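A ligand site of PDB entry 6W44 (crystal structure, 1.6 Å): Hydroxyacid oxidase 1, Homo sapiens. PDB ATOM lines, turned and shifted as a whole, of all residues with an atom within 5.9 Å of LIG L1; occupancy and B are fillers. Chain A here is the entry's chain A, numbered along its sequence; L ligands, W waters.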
ATOM      1  N   TYR A  26     -19.861 -24.456 -12.656  1.00  0.00           N
ATOM      2  CA  TYR A  26     -18.568 -24.539 -13.386  1.00  0.00           C
ATOM      3  C   TYR A  26     -17.552 -25.293 -12.522  1.00  0.00           C
ATOM      4  O   TYR A  26     -16.884 -26.269 -12.969  1.00  0.00           O
ATOM      5  CB  TYR A  26     -18.020 -23.164 -13.790  1.00  0.00           C
ATOM      6  CG  TYR A  26     -16.574 -23.262 -14.180  1.00  0.00           C
ATOM      7  CD1 TYR A  26     -16.179 -23.848 -15.369  1.00  0.00           C
ATOM      8  CD2 TYR A  26     -15.588 -22.807 -13.337  1.00  0.00           C
ATOM      9  CE1 TYR A  26     -14.838 -24.001 -15.672  1.00  0.00           C
ATOM     10  CE2 TYR A  26     -14.251 -22.886 -13.664  1.00  0.00           C
ATOM     11  CZ  TYR A  26     -13.868 -23.522 -14.815  1.00  0.00           C
ATOM     12  OH  TYR A  26     -12.532 -23.660 -15.033  1.00  0.00           O
ATOM     13  N   TYR A  27     -17.487 -24.937 -11.250  1.00  0.00           N
ATOM     14  CA  TYR A  27     -16.484 -25.561 -10.337  1.00  0.00           C
ATOM     15  C   TYR A  27     -16.869 -26.997 -10.016  1.00  0.00           C
ATOM     16  O   TYR A  27     -15.964 -27.863  -9.972  1.00  0.00           O
ATOM     17  CB  TYR A  27     -16.373 -24.717  -9.080  1.00  0.00           C
ATOM     18  CG  TYR A  27     -15.725 -23.375  -9.214  1.00  0.00           C
ATOM     19  CD1 TYR A  27     -14.546 -23.181  -9.906  1.00  0.00           C
ATOM     20  CD2 TYR A  27     -16.286 -22.282  -8.555  1.00  0.00           C
ATOM     21  CE1 TYR A  27     -13.916 -21.940  -9.943  1.00  0.00           C
ATOM     22  CE2 TYR A  27     -15.679 -21.046  -8.600  1.00  0.00           C
ATOM     23  CZ  TYR A  27     -14.496 -20.884  -9.271  1.00  0.00           C
ATOM     24  OH  TYR A  27     -13.826 -19.685  -9.320  1.00  0.00           O
ATOM     25  N   SER A  29     -18.825 -29.244 -11.574  1.00  0.00           N
ATOM     26  CA  SER A  29     -19.318 -30.159 -12.622  1.00  0.00           C
ATOM     27  C   SER A  29     -18.230 -31.152 -13.023  1.00  0.00           C
ATOM     28  O   SER A  29     -17.031 -30.854 -12.933  1.00  0.00           O
ATOM     29  CB  SER A  29     -19.835 -29.399 -13.822  1.00  0.00           C
ATOM     30  OG  SER A  29     -21.104 -28.863 -13.528  1.00  0.00           O
ATOM     31  N   ASN A  40     -14.710 -41.048  -8.330  1.00  0.00           N
ATOM     32  CA  ASN A  40     -13.488 -40.527  -7.676  1.00  0.00           C
ATOM     33  C   ASN A  40     -13.642 -40.521  -6.151  1.00  0.00           C
ATOM     34  O   ASN A  40     -12.668 -40.834  -5.441  1.00  0.00           O
ATOM     35  CB  ASN A  40     -13.111 -39.123  -8.166  1.00  0.00           C
ATOM     36  CG  ASN A  40     -12.330 -39.079  -9.467  1.00  0.00           C
ATOM     37  OD1 ASN A  40     -11.898 -40.157  -9.961  1.00  0.00           O
ATOM     38  ND2 ASN A  40     -12.106 -37.868 -10.001  1.00  0.00           N
ATOM     39  N   GLY A  78      -3.490 -28.297  -6.286  1.00  0.00           N
ATOM     40  CA  GLY A  78      -3.517 -28.497  -7.737  1.00  0.00           C
ATOM     41  C   GLY A  78      -3.940 -27.265  -8.519  1.00  0.00           C
ATOM     42  O   GLY A  78      -4.666 -26.396  -7.984  1.00  0.00           O
ATOM     43  N   ALA A  79      -3.648 -27.271  -9.810  1.00  0.00           N
ATOM     44  CA  ALA A  79      -3.996 -26.180 -10.739  1.00  0.00           C
ATOM     45  C   ALA A  79      -5.518 -26.089 -10.907  1.00  0.00           C
ATOM     46  O   ALA A  79      -6.161 -27.093 -11.268  1.00  0.00           O
ATOM     47  CB  ALA A  79      -3.325 -26.405 -12.061  1.00  0.00           C
ATOM     48  N   THR A  80      -6.104 -24.917 -10.731  1.00  0.00           N
ATOM     49  CA  THR A  80      -7.547 -24.692 -11.009  1.00  0.00           C
ATOM     50  C   THR A  80      -7.621 -23.317 -11.645  1.00  0.00           C
ATOM     51  O   THR A  80      -7.115 -22.352 -11.045  1.00  0.00           O
ATOM     52  CB  THR A  80      -8.471 -24.822  -9.796  1.00  0.00           C
ATOM     53  OG1 THR A  80      -7.970 -24.022  -8.714  1.00  0.00           O
ATOM     54  CG2 THR A  80      -8.629 -26.220  -9.276  1.00  0.00           C
ATOM     55  N   ALA A  81      -8.076 -23.238 -12.881  1.00  0.00           N
ATOM     56  CA  ALA A  81      -8.249 -21.975 -13.611  1.00  0.00           C
ATOM     57  C   ALA A  81      -9.307 -21.158 -12.870  1.00  0.00           C
ATOM     58  O   ALA A  81     -10.191 -21.722 -12.212  1.00  0.00           O
ATOM     59  CB  ALA A  81      -8.664 -22.245 -15.036  1.00  0.00           C
ATOM     60  N   MET A 106       0.640 -25.660  -7.310  1.00  0.00           N
ATOM     61  CA  MET A 106       0.661 -25.783  -8.770  1.00  0.00           C
ATOM     62  C   MET A 106      -0.224 -24.676  -9.371  1.00  0.00           C
ATOM     63  O   MET A 106      -1.440 -24.692  -9.152  1.00  0.00           O
ATOM     64  CB  MET A 106       0.137 -27.184  -9.179  1.00  0.00           C
ATOM     65  CG  MET A 106       0.428 -27.548 -10.616  1.00  0.00           C
ATOM     66  SD  MET A 106      -0.692 -28.852 -11.209  1.00  0.00           S
ATOM     67  CE  MET A 106      -0.380 -30.170 -10.040  1.00  0.00           C
ATOM     68  N   SER A 108      -2.058 -22.739 -12.346  1.00  0.00           N
ATOM     69  CA  SER A 108      -2.642 -23.031 -13.666  1.00  0.00           C
ATOM     70  C   SER A 108      -1.946 -22.149 -14.699  1.00  0.00           C
ATOM     71  O   SER A 108      -1.713 -21.021 -14.428  1.00  0.00           O
ATOM     72  CB  SER A 108      -4.106 -22.714 -13.678  1.00  0.00           C
ATOM     73  OG  SER A 108      -4.620 -22.786 -14.984  1.00  0.00           O
ATOM     74  N   SER A 109      -1.755 -22.638 -15.928  1.00  0.00           N
ATOM     75  CA  SER A 109      -1.250 -21.678 -16.940  1.00  0.00           C
ATOM     76  C   SER A 109      -2.363 -20.727 -17.414  1.00  0.00           C
ATOM     77  O   SER A 109      -2.027 -19.765 -18.044  1.00  0.00           O
ATOM     78  CB  SER A 109      -0.407 -22.284 -18.027  1.00  0.00           C
ATOM     79  OG  SER A 109      -1.142 -23.154 -18.798  1.00  0.00           O
ATOM     80  N   TRP A 110      -3.632 -20.986 -17.112  1.00  0.00           N
ATOM     81  CA  TRP A 110      -4.705 -19.989 -17.354  1.00  0.00           C
ATOM     82  C   TRP A 110      -5.020 -19.244 -16.049  1.00  0.00           C
ATOM     83  O   TRP A 110      -6.194 -19.009 -15.821  1.00  0.00           O
ATOM     84  CB  TRP A 110      -5.956 -20.665 -17.910  1.00  0.00           C
ATOM     85  CG  TRP A 110      -5.842 -21.057 -19.348  1.00  0.00           C
ATOM     86  CD1 TRP A 110      -5.322 -22.228 -19.816  1.00  0.00           C
ATOM     87  CD2 TRP A 110      -6.287 -20.326 -20.497  1.00  0.00           C
ATOM     88  NE1 TRP A 110      -5.408 -22.269 -21.173  1.00  0.00           N
ATOM     89  CE2 TRP A 110      -5.995 -21.114 -21.624  1.00  0.00           C
ATOM     90  CE3 TRP A 110      -6.899 -19.081 -20.690  1.00  0.00           C
ATOM     91  CZ2 TRP A 110      -6.283 -20.700 -22.925  1.00  0.00           C
ATOM     92  CZ3 TRP A 110      -7.187 -18.671 -21.977  1.00  0.00           C
ATOM     93  CH2 TRP A 110      -6.884 -19.470 -23.070  1.00  0.00           C
ATOM     94  N   GLN A 130       1.790 -25.428 -13.905  1.00  0.00           N
ATOM     95  CA  GLN A 130       1.078 -26.352 -14.808  1.00  0.00           C
ATOM     96  C   GLN A 130       1.089 -25.711 -16.196  1.00  0.00           C
ATOM     97  O   GLN A 130       0.866 -24.482 -16.299  1.00  0.00           O
ATOM     98  CB  GLN A 130      -0.346 -26.582 -14.330  1.00  0.00           C
ATOM     99  CG  GLN A 130      -1.200 -27.387 -15.295  1.00  0.00           C
ATOM    100  CD  GLN A 130      -1.850 -26.647 -16.427  1.00  0.00           C
ATOM    101  OE1 GLN A 130      -1.887 -27.103 -17.595  1.00  0.00           O
ATOM    102  NE2 GLN A 130      -2.532 -25.590 -16.062  1.00  0.00           N
ATOM    103  N   TYR A 132       0.082 -26.155 -20.453  1.00  0.00           N
ATOM    104  CA  TYR A 132      -0.484 -26.785 -21.665  1.00  0.00           C
ATOM    105  C   TYR A 132       0.506 -26.474 -22.786  1.00  0.00           C
ATOM    106  O   TYR A 132       1.119 -25.340 -22.749  1.00  0.00           O
ATOM    107  CB  TYR A 132      -1.842 -26.208 -22.048  1.00  0.00           C
ATOM    108  CG  TYR A 132      -2.951 -26.638 -21.119  1.00  0.00           C
ATOM    109  CD1 TYR A 132      -3.370 -27.947 -21.182  1.00  0.00           C
ATOM    110  CD2 TYR A 132      -3.594 -25.762 -20.268  1.00  0.00           C
ATOM    111  CE1 TYR A 132      -4.404 -28.386 -20.373  1.00  0.00           C
ATOM    112  CE2 TYR A 132      -4.624 -26.188 -19.441  1.00  0.00           C
ATOM    113  CZ  TYR A 132      -5.042 -27.503 -19.527  1.00  0.00           C
ATOM    114  OH  TYR A 132      -6.056 -28.006 -18.721  1.00  0.00           O
ATOM    115  N   THR A 158       0.099 -30.907 -18.640  1.00  0.00           N
ATOM    116  CA  THR A 158      -1.219 -31.586 -18.692  1.00  0.00           C
ATOM    117  C   THR A 158      -1.340 -32.290 -20.029  1.00  0.00           C
ATOM    118  O   THR A 158      -1.205 -31.607 -21.076  1.00  0.00           O
ATOM    119  CB  THR A 158      -2.354 -30.607 -18.404  1.00  0.00           C
ATOM    120  OG1 THR A 158      -2.145 -30.027 -17.131  1.00  0.00           O
ATOM    121  CG2 THR A 158      -3.675 -31.323 -18.430  1.00  0.00           C
ATOM    122  N   LYS A 236       0.907 -34.913 -16.185  1.00  0.00           N
ATOM    123  CA  LYS A 236      -0.368 -34.834 -15.427  1.00  0.00           C
ATOM    124  C   LYS A 236      -1.521 -35.342 -16.305  1.00  0.00           C
ATOM    125  O   LYS A 236      -1.761 -34.722 -17.361  1.00  0.00           O
ATOM    126  CB  LYS A 236      -0.580 -33.381 -15.009  1.00  0.00           C
ATOM    127  CG  LYS A 236      -1.925 -33.095 -14.379  1.00  0.00           C
ATOM    128  CD  LYS A 236      -2.002 -31.647 -13.933  1.00  0.00           C
ATOM    129  CE  LYS A 236      -3.264 -31.279 -13.150  1.00  0.00           C
ATOM    130  NZ  LYS A 236      -4.462 -31.229 -13.996  1.00  0.00           N
ATOM    131  N   SER A 258      -4.291 -38.727 -12.741  1.00  0.00           N
ATOM    132  CA  SER A 258      -5.339 -37.678 -12.720  1.00  0.00           C
ATOM    133  C   SER A 258      -6.312 -37.987 -13.846  1.00  0.00           C
ATOM    134  O   SER A 258      -5.878 -38.407 -14.933  1.00  0.00           O
ATOM    135  CB  SER A 258      -4.727 -36.315 -12.901  1.00  0.00           C
ATOM    136  OG  SER A 258      -5.741 -35.293 -12.917  1.00  0.00           O
ATOM    137  N   ASN A 259      -7.604 -37.745 -13.594  1.00  0.00           N
ATOM    138  CA  ASN A 259      -8.638 -37.738 -14.642  1.00  0.00           C
ATOM    139  C   ASN A 259      -9.185 -36.313 -14.742  1.00  0.00           C
ATOM    140  O   ASN A 259     -10.313 -36.136 -15.181  1.00  0.00           O
ATOM    141  CB  ASN A 259      -9.709 -38.813 -14.441  1.00  0.00           C
ATOM    142  CG  ASN A 259     -10.294 -38.861 -13.054  1.00  0.00           C
ATOM    143  OD1 ASN A 259     -10.449 -37.785 -12.452  1.00  0.00           O
ATOM    144  ND2 ASN A 259     -10.655 -40.039 -12.555  1.00  0.00           N
ATOM    145  N   HIS A 260      -8.395 -35.335 -14.330  1.00  0.00           N
ATOM    146  CA  HIS A 260      -8.743 -33.893 -14.515  1.00  0.00           C
ATOM    147  C   HIS A 260      -9.974 -33.599 -13.663  1.00  0.00           C
ATOM    148  O   HIS A 260     -10.887 -32.841 -14.123  1.00  0.00           O
ATOM    149  CB  HIS A 260      -8.946 -33.547 -15.995  1.00  0.00           C
ATOM    150  CG  HIS A 260      -8.643 -32.142 -16.339  1.00  0.00           C
ATOM    151  ND1 HIS A 260      -7.556 -31.797 -17.136  1.00  0.00           N
ATOM    152  CD2 HIS A 260      -9.330 -30.972 -16.097  1.00  0.00           C
ATOM    153  CE1 HIS A 260      -7.586 -30.464 -17.351  1.00  0.00           C
ATOM    154  NE2 HIS A 260      -8.630 -29.943 -16.725  1.00  0.00           N
ATOM    155  N   GLY A 261     -10.070 -34.211 -12.480  1.00  0.00           N
ATOM    156  CA  GLY A 261     -11.240 -33.991 -11.604  1.00  0.00           C
ATOM    157  C   GLY A 261     -12.523 -34.485 -12.265  1.00  0.00           C
ATOM    158  O   GLY A 261     -13.613 -33.969 -11.992  1.00  0.00           O
ATOM    159  N   ALA A 262     -12.432 -35.504 -13.094  1.00  0.00           N
ATOM    160  CA  ALA A 262     -13.560 -36.147 -13.803  1.00  0.00           C
ATOM    161  C   ALA A 262     -14.216 -35.179 -14.801  1.00  0.00           C
ATOM    162  O   ALA A 262     -15.396 -35.347 -15.097  1.00  0.00           O
ATOM    163  CB  ALA A 262     -14.540 -36.687 -12.794  1.00  0.00           C
ATOM    164  N   ARG A 263     -13.467 -34.231 -15.370  1.00  0.00           N
ATOM    165  CA  ARG A 263     -14.001 -33.153 -16.237  1.00  0.00           C
ATOM    166  C   ARG A 263     -13.684 -33.397 -17.708  1.00  0.00           C
ATOM    167  O   ARG A 263     -14.118 -32.600 -18.541  1.00  0.00           O
ATOM    168  CB  ARG A 263     -13.460 -31.811 -15.756  1.00  0.00           C
ATOM    169  CG  ARG A 263     -13.935 -31.458 -14.358  1.00  0.00           C
ATOM    170  CD  ARG A 263     -13.112 -30.330 -13.759  1.00  0.00           C
ATOM    171  NE  ARG A 263     -13.307 -29.025 -14.355  1.00  0.00           N
ATOM    172  CZ  ARG A 263     -14.265 -28.173 -13.962  1.00  0.00           C
ATOM    173  NH1 ARG A 263     -15.192 -28.549 -13.108  1.00  0.00           N
ATOM    174  NH2 ARG A 263     -14.262 -26.940 -14.424  1.00  0.00           N
ATOM    175  N   ASP A 291      -4.416 -37.033  -7.934  1.00  0.00           N
ATOM    176  CA  ASP A 291      -5.518 -36.090  -7.605  1.00  0.00           C
ATOM    177  C   ASP A 291      -6.840 -36.744  -8.023  1.00  0.00           C
ATOM    178  O   ASP A 291      -6.829 -37.757  -8.740  1.00  0.00           O
ATOM    179  CB  ASP A 291      -5.305 -34.694  -8.184  1.00  0.00           C
ATOM    180  CG  ASP A 291      -5.362 -34.527  -9.684  1.00  0.00           C
ATOM    181  OD1 ASP A 291      -6.058 -35.361 -10.343  1.00  0.00           O
ATOM    182  OD2 ASP A 291      -4.789 -33.542 -10.177  1.00  0.00           O
ATOM    183  N   GLY A 292      -7.976 -36.131  -7.643  1.00  0.00           N
ATOM    184  CA  GLY A 292      -9.273 -36.630  -8.020  1.00  0.00           C
ATOM    185  C   GLY A 292      -9.969 -37.206  -6.810  1.00  0.00           C
ATOM    186  O   GLY A 292      -9.755 -38.335  -6.475  1.00  0.00           O
ATOM    187  N   GLY A 293     -10.855 -36.430  -6.189  1.00  0.00           N
ATOM    188  CA  GLY A 293     -11.697 -36.962  -5.135  1.00  0.00           C
ATOM    189  C   GLY A 293     -11.114 -36.863  -3.735  1.00  0.00           C
ATOM    190  O   GLY A 293     -11.753 -37.398  -2.836  1.00  0.00           O
ATOM    191  N   VAL A 294      -9.946 -36.271  -3.530  1.00  0.00           N
ATOM    192  CA  VAL A 294      -9.381 -36.149  -2.175  1.00  0.00           C
ATOM    193  C   VAL A 294     -10.206 -35.117  -1.399  1.00  0.00           C
ATOM    194  O   VAL A 294     -10.210 -33.971  -1.825  1.00  0.00           O
ATOM    195  CB  VAL A 294      -7.886 -35.809  -2.229  1.00  0.00           C
ATOM    196  CG1 VAL A 294      -7.340 -35.600  -0.843  1.00  0.00           C
ATOM    197  CG2 VAL A 294      -7.112 -36.899  -2.977  1.00  0.00           C
ATOM    198  N   ARG A 295     -10.829 -35.560  -0.307  1.00  0.00           N
ATOM    199  CA  ARG A 295     -11.699 -34.686   0.529  1.00  0.00           C
ATOM    200  C   ARG A 295     -11.408 -34.861   2.004  1.00  0.00           C
ATOM    201  O   ARG A 295     -11.824 -34.010   2.767  1.00  0.00           O
ATOM    202  CB  ARG A 295     -13.144 -35.019   0.263  1.00  0.00           C
ATOM    203  CG  ARG A 295     -13.614 -34.911  -1.185  1.00  0.00           C
ATOM    204  CD  ARG A 295     -13.562 -33.499  -1.716  1.00  0.00           C
ATOM    205  NE  ARG A 295     -13.989 -33.415  -3.133  1.00  0.00           N
ATOM    206  CZ  ARG A 295     -13.166 -33.395  -4.192  1.00  0.00           C
ATOM    207  NH1 ARG A 295     -11.850 -33.383  -4.040  1.00  0.00           N
ATOM    208  NH2 ARG A 295     -13.683 -33.340  -5.405  1.00  0.00           N
ATOM    209  N   PHE A 312      -2.797 -34.109  -4.634  1.00  0.00           N
ATOM    210  CA  PHE A 312      -3.187 -32.719  -4.935  1.00  0.00           C
ATOM    211  C   PHE A 312      -4.681 -32.600  -4.795  1.00  0.00           C
ATOM    212  O   PHE A 312      -5.438 -33.556  -5.062  1.00  0.00           O
ATOM    213  CB  PHE A 312      -2.758 -32.320  -6.345  1.00  0.00           C
ATOM    214  CG  PHE A 312      -1.270 -32.247  -6.536  1.00  0.00           C
ATOM    215  CD1 PHE A 312      -0.528 -33.408  -6.717  1.00  0.00           C
ATOM    216  CD2 PHE A 312      -0.609 -31.039  -6.495  1.00  0.00           C
ATOM    217  CE1 PHE A 312       0.861 -33.354  -6.825  1.00  0.00           C
ATOM    218  CE2 PHE A 312       0.776 -30.991  -6.648  1.00  0.00           C
ATOM    219  CZ  PHE A 312       1.504 -32.145  -6.798  1.00  0.00           C
ATOM    220  N   VAL A 313      -5.108 -31.410  -4.381  1.00  0.00           N
ATOM    221  CA  VAL A 313      -6.555 -31.073  -4.249  1.00  0.00           C
ATOM    222  C   VAL A 313      -6.889 -29.913  -5.175  1.00  0.00           C
ATOM    223  O   VAL A 313      -6.111 -28.947  -5.235  1.00  0.00           O
ATOM    224  CB  VAL A 313      -6.975 -30.748  -2.814  1.00  0.00           C
ATOM    225  CG1 VAL A 313      -7.081 -32.040  -1.980  1.00  0.00           C
ATOM    226  CG2 VAL A 313      -6.050 -29.744  -2.176  1.00  0.00           C
ATOM    227  N   GLY A 314      -8.009 -30.038  -5.885  1.00  0.00           N
ATOM    228  CA  GLY A 314      -8.503 -28.995  -6.790  1.00  0.00           C
ATOM    229  C   GLY A 314      -9.658 -28.249  -6.184  1.00  0.00           C
ATOM    230  O   GLY A 314      -9.484 -27.194  -5.588  1.00  0.00           O
ATOM    231  N   ARG A 315     -10.832 -28.819  -6.280  1.00  0.00           N
ATOM    232  CA  ARG A 315     -12.079 -28.124  -5.870  1.00  0.00           C
ATOM    233  C   ARG A 315     -12.001 -27.650  -4.412  1.00  0.00           C
ATOM    234  O   ARG A 315     -12.537 -26.563  -4.164  1.00  0.00           O
ATOM    235  CB  ARG A 315     -13.283 -29.013  -6.096  1.00  0.00           C
ATOM    236  CG  ARG A 315     -13.661 -29.194  -7.563  1.00  0.00           C
ATOM    237  CD  ARG A 315     -14.795 -30.132  -7.779  1.00  0.00           C
ATOM    238  NE  ARG A 315     -15.057 -30.422  -9.159  1.00  0.00           N
ATOM    239  CZ  ARG A 315     -14.542 -31.428  -9.832  1.00  0.00           C
ATOM    240  NH1 ARG A 315     -13.628 -32.172  -9.265  1.00  0.00           N
ATOM    241  NH2 ARG A 315     -14.971 -31.678 -11.068  1.00  0.00           N
ATOM    242  N   PRO A 316     -11.461 -28.400  -3.429  1.00  0.00           N
ATOM    243  CA  PRO A 316     -11.483 -27.952  -2.021  1.00  0.00           C
ATOM    244  C   PRO A 316     -10.874 -26.557  -1.863  1.00  0.00           C
ATOM    245  O   PRO A 316     -11.393 -25.774  -1.059  1.00  0.00           O
ATOM    246  CB  PRO A 316     -10.688 -29.026  -1.286  1.00  0.00           C
ATOM    247  CG  PRO A 316     -11.080 -30.280  -2.081  1.00  0.00           C
ATOM    248  CD  PRO A 316     -10.965 -29.795  -3.518  1.00  0.00           C
ATOM    249  N   VAL A 318     -10.839 -24.080  -4.137  1.00  0.00           N
ATOM    250  CA  VAL A 318     -11.828 -23.122  -4.668  1.00  0.00           C
ATOM    251  C   VAL A 318     -12.901 -22.889  -3.599  1.00  0.00           C
ATOM    252  O   VAL A 318     -13.327 -21.738  -3.407  1.00  0.00           O
ATOM    253  CB  VAL A 318     -12.434 -23.650  -5.977  1.00  0.00           C
ATOM    254  CG1 VAL A 318     -13.538 -22.726  -6.422  1.00  0.00           C
ATOM    255  CG2 VAL A 318     -11.366 -23.806  -7.033  1.00  0.00           C
HETATM  256  N1  LIG L   1      -6.000 -28.779 -14.463  1.00  0.00           N
HETATM  257  C1  LIG L   1      -5.058 -28.182 -15.244  1.00  0.00           C
HETATM  258  O1  LIG L   1      -4.056 -28.851 -15.580  1.00  0.00           O
HETATM  259  N2  LIG L   1      -5.154 -26.914 -15.666  1.00  0.00           N
HETATM  260  C2  LIG L   1      -6.194 -26.135 -15.345  1.00  0.00           C
HETATM  261  O2  LIG L   1      -6.256 -24.950 -15.760  1.00  0.00           O
HETATM  262  C3  LIG L   1      -7.271 -26.695 -14.502  1.00  0.00           C
HETATM  263  N3  LIG L   1      -8.357 -25.975 -14.130  1.00  0.00           N
HETATM  264  C4  LIG L   1      -9.322 -26.524 -13.351  1.00  0.00           C
HETATM  265  C5  LIG L   1     -10.430 -25.766 -12.990  1.00  0.00           C
HETATM  266  C6  LIG L   1     -11.413 -26.320 -12.198  1.00  0.00           C
HETATM  267  C7  LIG L   1     -12.613 -25.490 -11.803  1.00  0.00           C
HETATM  268  C8  LIG L   1     -11.306 -27.730 -11.733  1.00  0.00           C
HETATM  269  C9  LIG L   1     -12.384 -28.328 -10.864  1.00  0.00           C
HETATM  270  C10 LIG L   1     -10.198 -28.489 -12.093  1.00  0.00           C
HETATM  271  C11 LIG L   1      -9.208 -27.941 -12.888  1.00  0.00           C
HETATM  272  N4  LIG L   1      -8.081 -28.707 -13.258  1.00  0.00           N
HETATM  273  C12 LIG L   1      -7.098 -28.105 -14.067  1.00  0.00           C
HETATM  274  C13 LIG L   1      -7.953 -30.091 -12.815  1.00  0.00           C
HETATM  275  C14 LIG L   1      -7.228 -30.123 -11.472  1.00  0.00           C
HETATM  276  O3  LIG L   1      -5.865 -29.722 -11.649  1.00  0.00           O
HETATM  277  C15 LIG L   1      -7.284 -31.519 -10.857  1.00  0.00           C
HETATM  278  O4  LIG L   1      -6.985 -32.487 -11.863  1.00  0.00           O
HETATM  279  C16 LIG L   1      -8.646 -31.809 -10.248  1.00  0.00           C
HETATM  280  O5  LIG L   1      -9.270 -30.577  -9.859  1.00  0.00           O
HETATM  281  C17 LIG L   1      -8.527 -32.729  -9.045  1.00  0.00           C
HETATM  282  O6  LIG L   1      -9.826 -33.214  -8.694  1.00  0.00           O
HETATM  283  P1  LIG L   1     -10.590 -32.631  -7.401  1.00  0.00           P
HETATM  284  O7  LIG L   1      -9.490 -32.471  -6.367  1.00  0.00           O
HETATM  285  O8  LIG L   1     -11.602 -33.698  -7.068  1.00  0.00           O
HETATM  286  O9  LIG L   1     -11.184 -31.331  -7.886  1.00  0.00           O
HETATM  287  C1  LG2 L   2     -15.499 -19.694 -15.361  1.00  0.00           C
HETATM  288  C2  LG2 L   2     -15.729 -20.442 -16.562  1.00  0.00           C
HETATM  289  C3  LG2 L   2     -14.358 -21.537 -18.141  1.00  0.00           C
HETATM  290  C4  LG2 L   2     -13.034 -21.883 -18.575  1.00  0.00           C
HETATM  291  C5  LG2 L   2     -11.828 -21.403 -17.822  1.00  0.00           C
HETATM  292  C6  LG2 L   2      -9.837 -20.433 -19.063  1.00  0.00           C
HETATM  293  C7  LG2 L   2      -9.880 -22.834 -18.350  1.00  0.00           C
HETATM  294  C8  LG2 L   2     -10.514 -23.911 -17.735  1.00  0.00           C
HETATM  295  C9  LG2 L   2      -9.806 -25.113 -17.620  1.00  0.00           C
HETATM  296  C10 LG2 L   2      -8.500 -25.220 -18.114  1.00  0.00           C
HETATM  297  C11 LG2 L   2     -10.079 -26.391 -17.067  1.00  0.00           C
HETATM  298  C12 LG2 L   2     -11.292 -26.853 -16.395  1.00  0.00           C
HETATM  299  C13 LG2 L   2      -7.879 -24.161 -18.763  1.00  0.00           C
HETATM  300  O1  LG2 L   2     -12.266 -26.102 -16.206  1.00  0.00           O
HETATM  301  O2  LG2 L   2     -11.322 -28.110 -16.094  1.00  0.00           O
HETATM  302  N1  LG2 L   2      -9.039 -27.214 -17.225  1.00  0.00           N
HETATM  303  N2  LG2 L   2      -8.079 -26.488 -17.839  1.00  0.00           N
HETATM  304  C14 LG2 L   2      -8.598 -22.972 -18.868  1.00  0.00           C
HETATM  305  N3  LG2 L   2     -10.541 -21.591 -18.499  1.00  0.00           N
HETATM  306  C15 LG2 L   2     -12.973 -22.697 -19.693  1.00  0.00           C
HETATM  307  C16 LG2 L   2     -14.135 -23.150 -20.285  1.00  0.00           C
HETATM  308  C17 LG2 L   2     -15.347 -22.749 -19.756  1.00  0.00           C
HETATM  309  N4  LG2 L   2     -15.470 -21.937 -18.697  1.00  0.00           N
HETATM  310  O3  LG2 L   2     -14.409 -20.797 -17.028  1.00  0.00           O
HETATM  311  C18 LG2 L   2     -16.890 -19.419 -14.697  1.00  0.00           C
HETATM  312  O   HOH W   1      -8.113 -34.443  -5.369  1.00  0.00           O
HETATM  313  O   HOH W   2      -3.973 -30.906  -9.783  1.00  0.00           O
HETATM  314  O   HOH W   3     -12.889 -35.292  -8.915  1.00  0.00           O
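N3 of LIG L1 lies close to N1 of LG2 L2, 3.4 Å away.
N2 of LG2 L2 lies within hydrogen-bond range of OH of Tyr 132.
An oxygen (O9) of LIG L1 sits at hydrogen-bond distance from the backbone NH of Arg 315 (3.0 Å).
The side-chain amino group (NZ) of Lys 236 is in hydrogen-bond range of an oxygen (O1) of LIG L1, 2.9 Å away.
The guanidinium group (NH2) of Arg 295 lies within salt-bridge range of an oxygen (O8) of LIG L1, at 2.7 Å.
An oxygen (O8) of LIG L1 sits at hydrogen-bond distance from the backbone NH (N) of Gly 293 (3.0 Å).
OH of Tyr 132 sits at hydrogen-bond distance from N2 of LIG L1.
An oxygen (O9) of LIG L1 is in salt-bridge range of the guanidinium group (NH1) of Arg 315, 2.9 Å away.
The backbone NH (N) of Ala 81 lies within hydrogen-bond range of a nitrogen (N3) of LIG L1 (3.0 Å).
An oxygen (O7) of LIG L1 lies within hydrogen-bond range of the backbone NH of Gly 314, 2.9 Å away.
OG1 of Thr 158 lies within hydrogen-bond range of O1 of LIG L1 (2.7 Å).
A ring nitrogen (NE2) of His 260 lies within hydrogen-bond range of a nitrogen (N1) of LG2 L2, at 2.8 Å.
O4 of LIG L1 sits at hydrogen-bond distance from OG of Ser 258, 3.2 Å away.
The guanidinium group (NE) of Arg 263 lies within salt-bridge range of an oxygen (O2) of LG2 L2, at 2.8 Å.
O1 of LG2 L2 sits at hydrogen-bond distance from OH of Tyr 26, at 2.7 Å.
The backbone carbonyl oxygen (O) of Ala 79 sits at hydrogen-bond distance from an oxygen (O3) of LIG L1, 2.7 Å away.
The side-chain amide nitrogen (NE2) of Gln 130 sits close to a nitrogen (N2) of LIG L1 (3.0 Å).
The side-chain carboxylate of Asp 291 is in hydrogen-bond range of an oxygen (O4) of LIG L1 (3.0 Å).
The side-chain hydroxyl of Ser 108 lies within hydrogen-bond range of an oxygen (O2) of LIG L1.
CE2 of Tyr 26 touches C7 of LIG L1, 3.6 Å away.
Tyr 27 touches LIG L1 (CD1 to C7, 3.6 Å).
Thr 80 touches LIG L1.
His 260 touches LIG L1.
CA of Gly 261 touches O6 of LIG L1 (3.3 Å).
Arg 263 touches LIG L1 (NH2 to C7, 3.4 Å).
CA of Gly 292 touches O6 of LIG L1, at 3.5 Å.
Val 313 touches LIG L1 (C to O7, 3.8 Å).
Hydrophobic or aromatic side chains that line LIG L1: Tyr 26, Tyr 27, Ala 81, Tyr 132 and His 260.
The nearest printed residue that does not touch LIG L1 is Pro 316 (4.2 Å).
The backbone carbonyl oxygen (O) of Ser 29 sits at hydrogen-bond distance from the guanidinium group (NH2) of Arg 315.
The backbone carbonyl oxygen (O) of Ser 29 sits at hydrogen-bond distance from the guanidinium group (NH1) of Arg 263 (3.0 Å).
O of Val 313 is in hydrogen-bond range of N of Gly 78 (2.9 Å).
OG1 of Thr 158 lies within hydrogen-bond range of OE1 of Gln 130 (3.0 Å).
The guanidinium group (NE) of Arg 315 lies within hydrogen-bond range of the backbone carbonyl oxygen (O) of Tyr 27 (2.8 Å).
O of Met 106 lies close to N of Ala 79.
The guanidinium group of Arg 315 sits at hydrogen-bond distance from the backbone carbonyl oxygen of Gly 261 (2.8 Å).
NE2 of Gln 130 lies close to N of Ser 109, 3.1 Å away.
Water W3 lies within hydrogen-bond range of an oxygen (O8) of LIG L1 (2.8 Å), the side-chain amide nitrogen (ND2) of Asn 40 (2.9 Å), the guanidinium group (NH1) of Arg 315 (3.2 Å) and the backbone carbonyl oxygen (O) of Gly 261 (3.4 Å).
Water W2 bridges the side-chain carboxylate (OD2) of Asp 291 (2.8 Å) and an oxygen (O3) of LIG L1 (2.9 Å).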
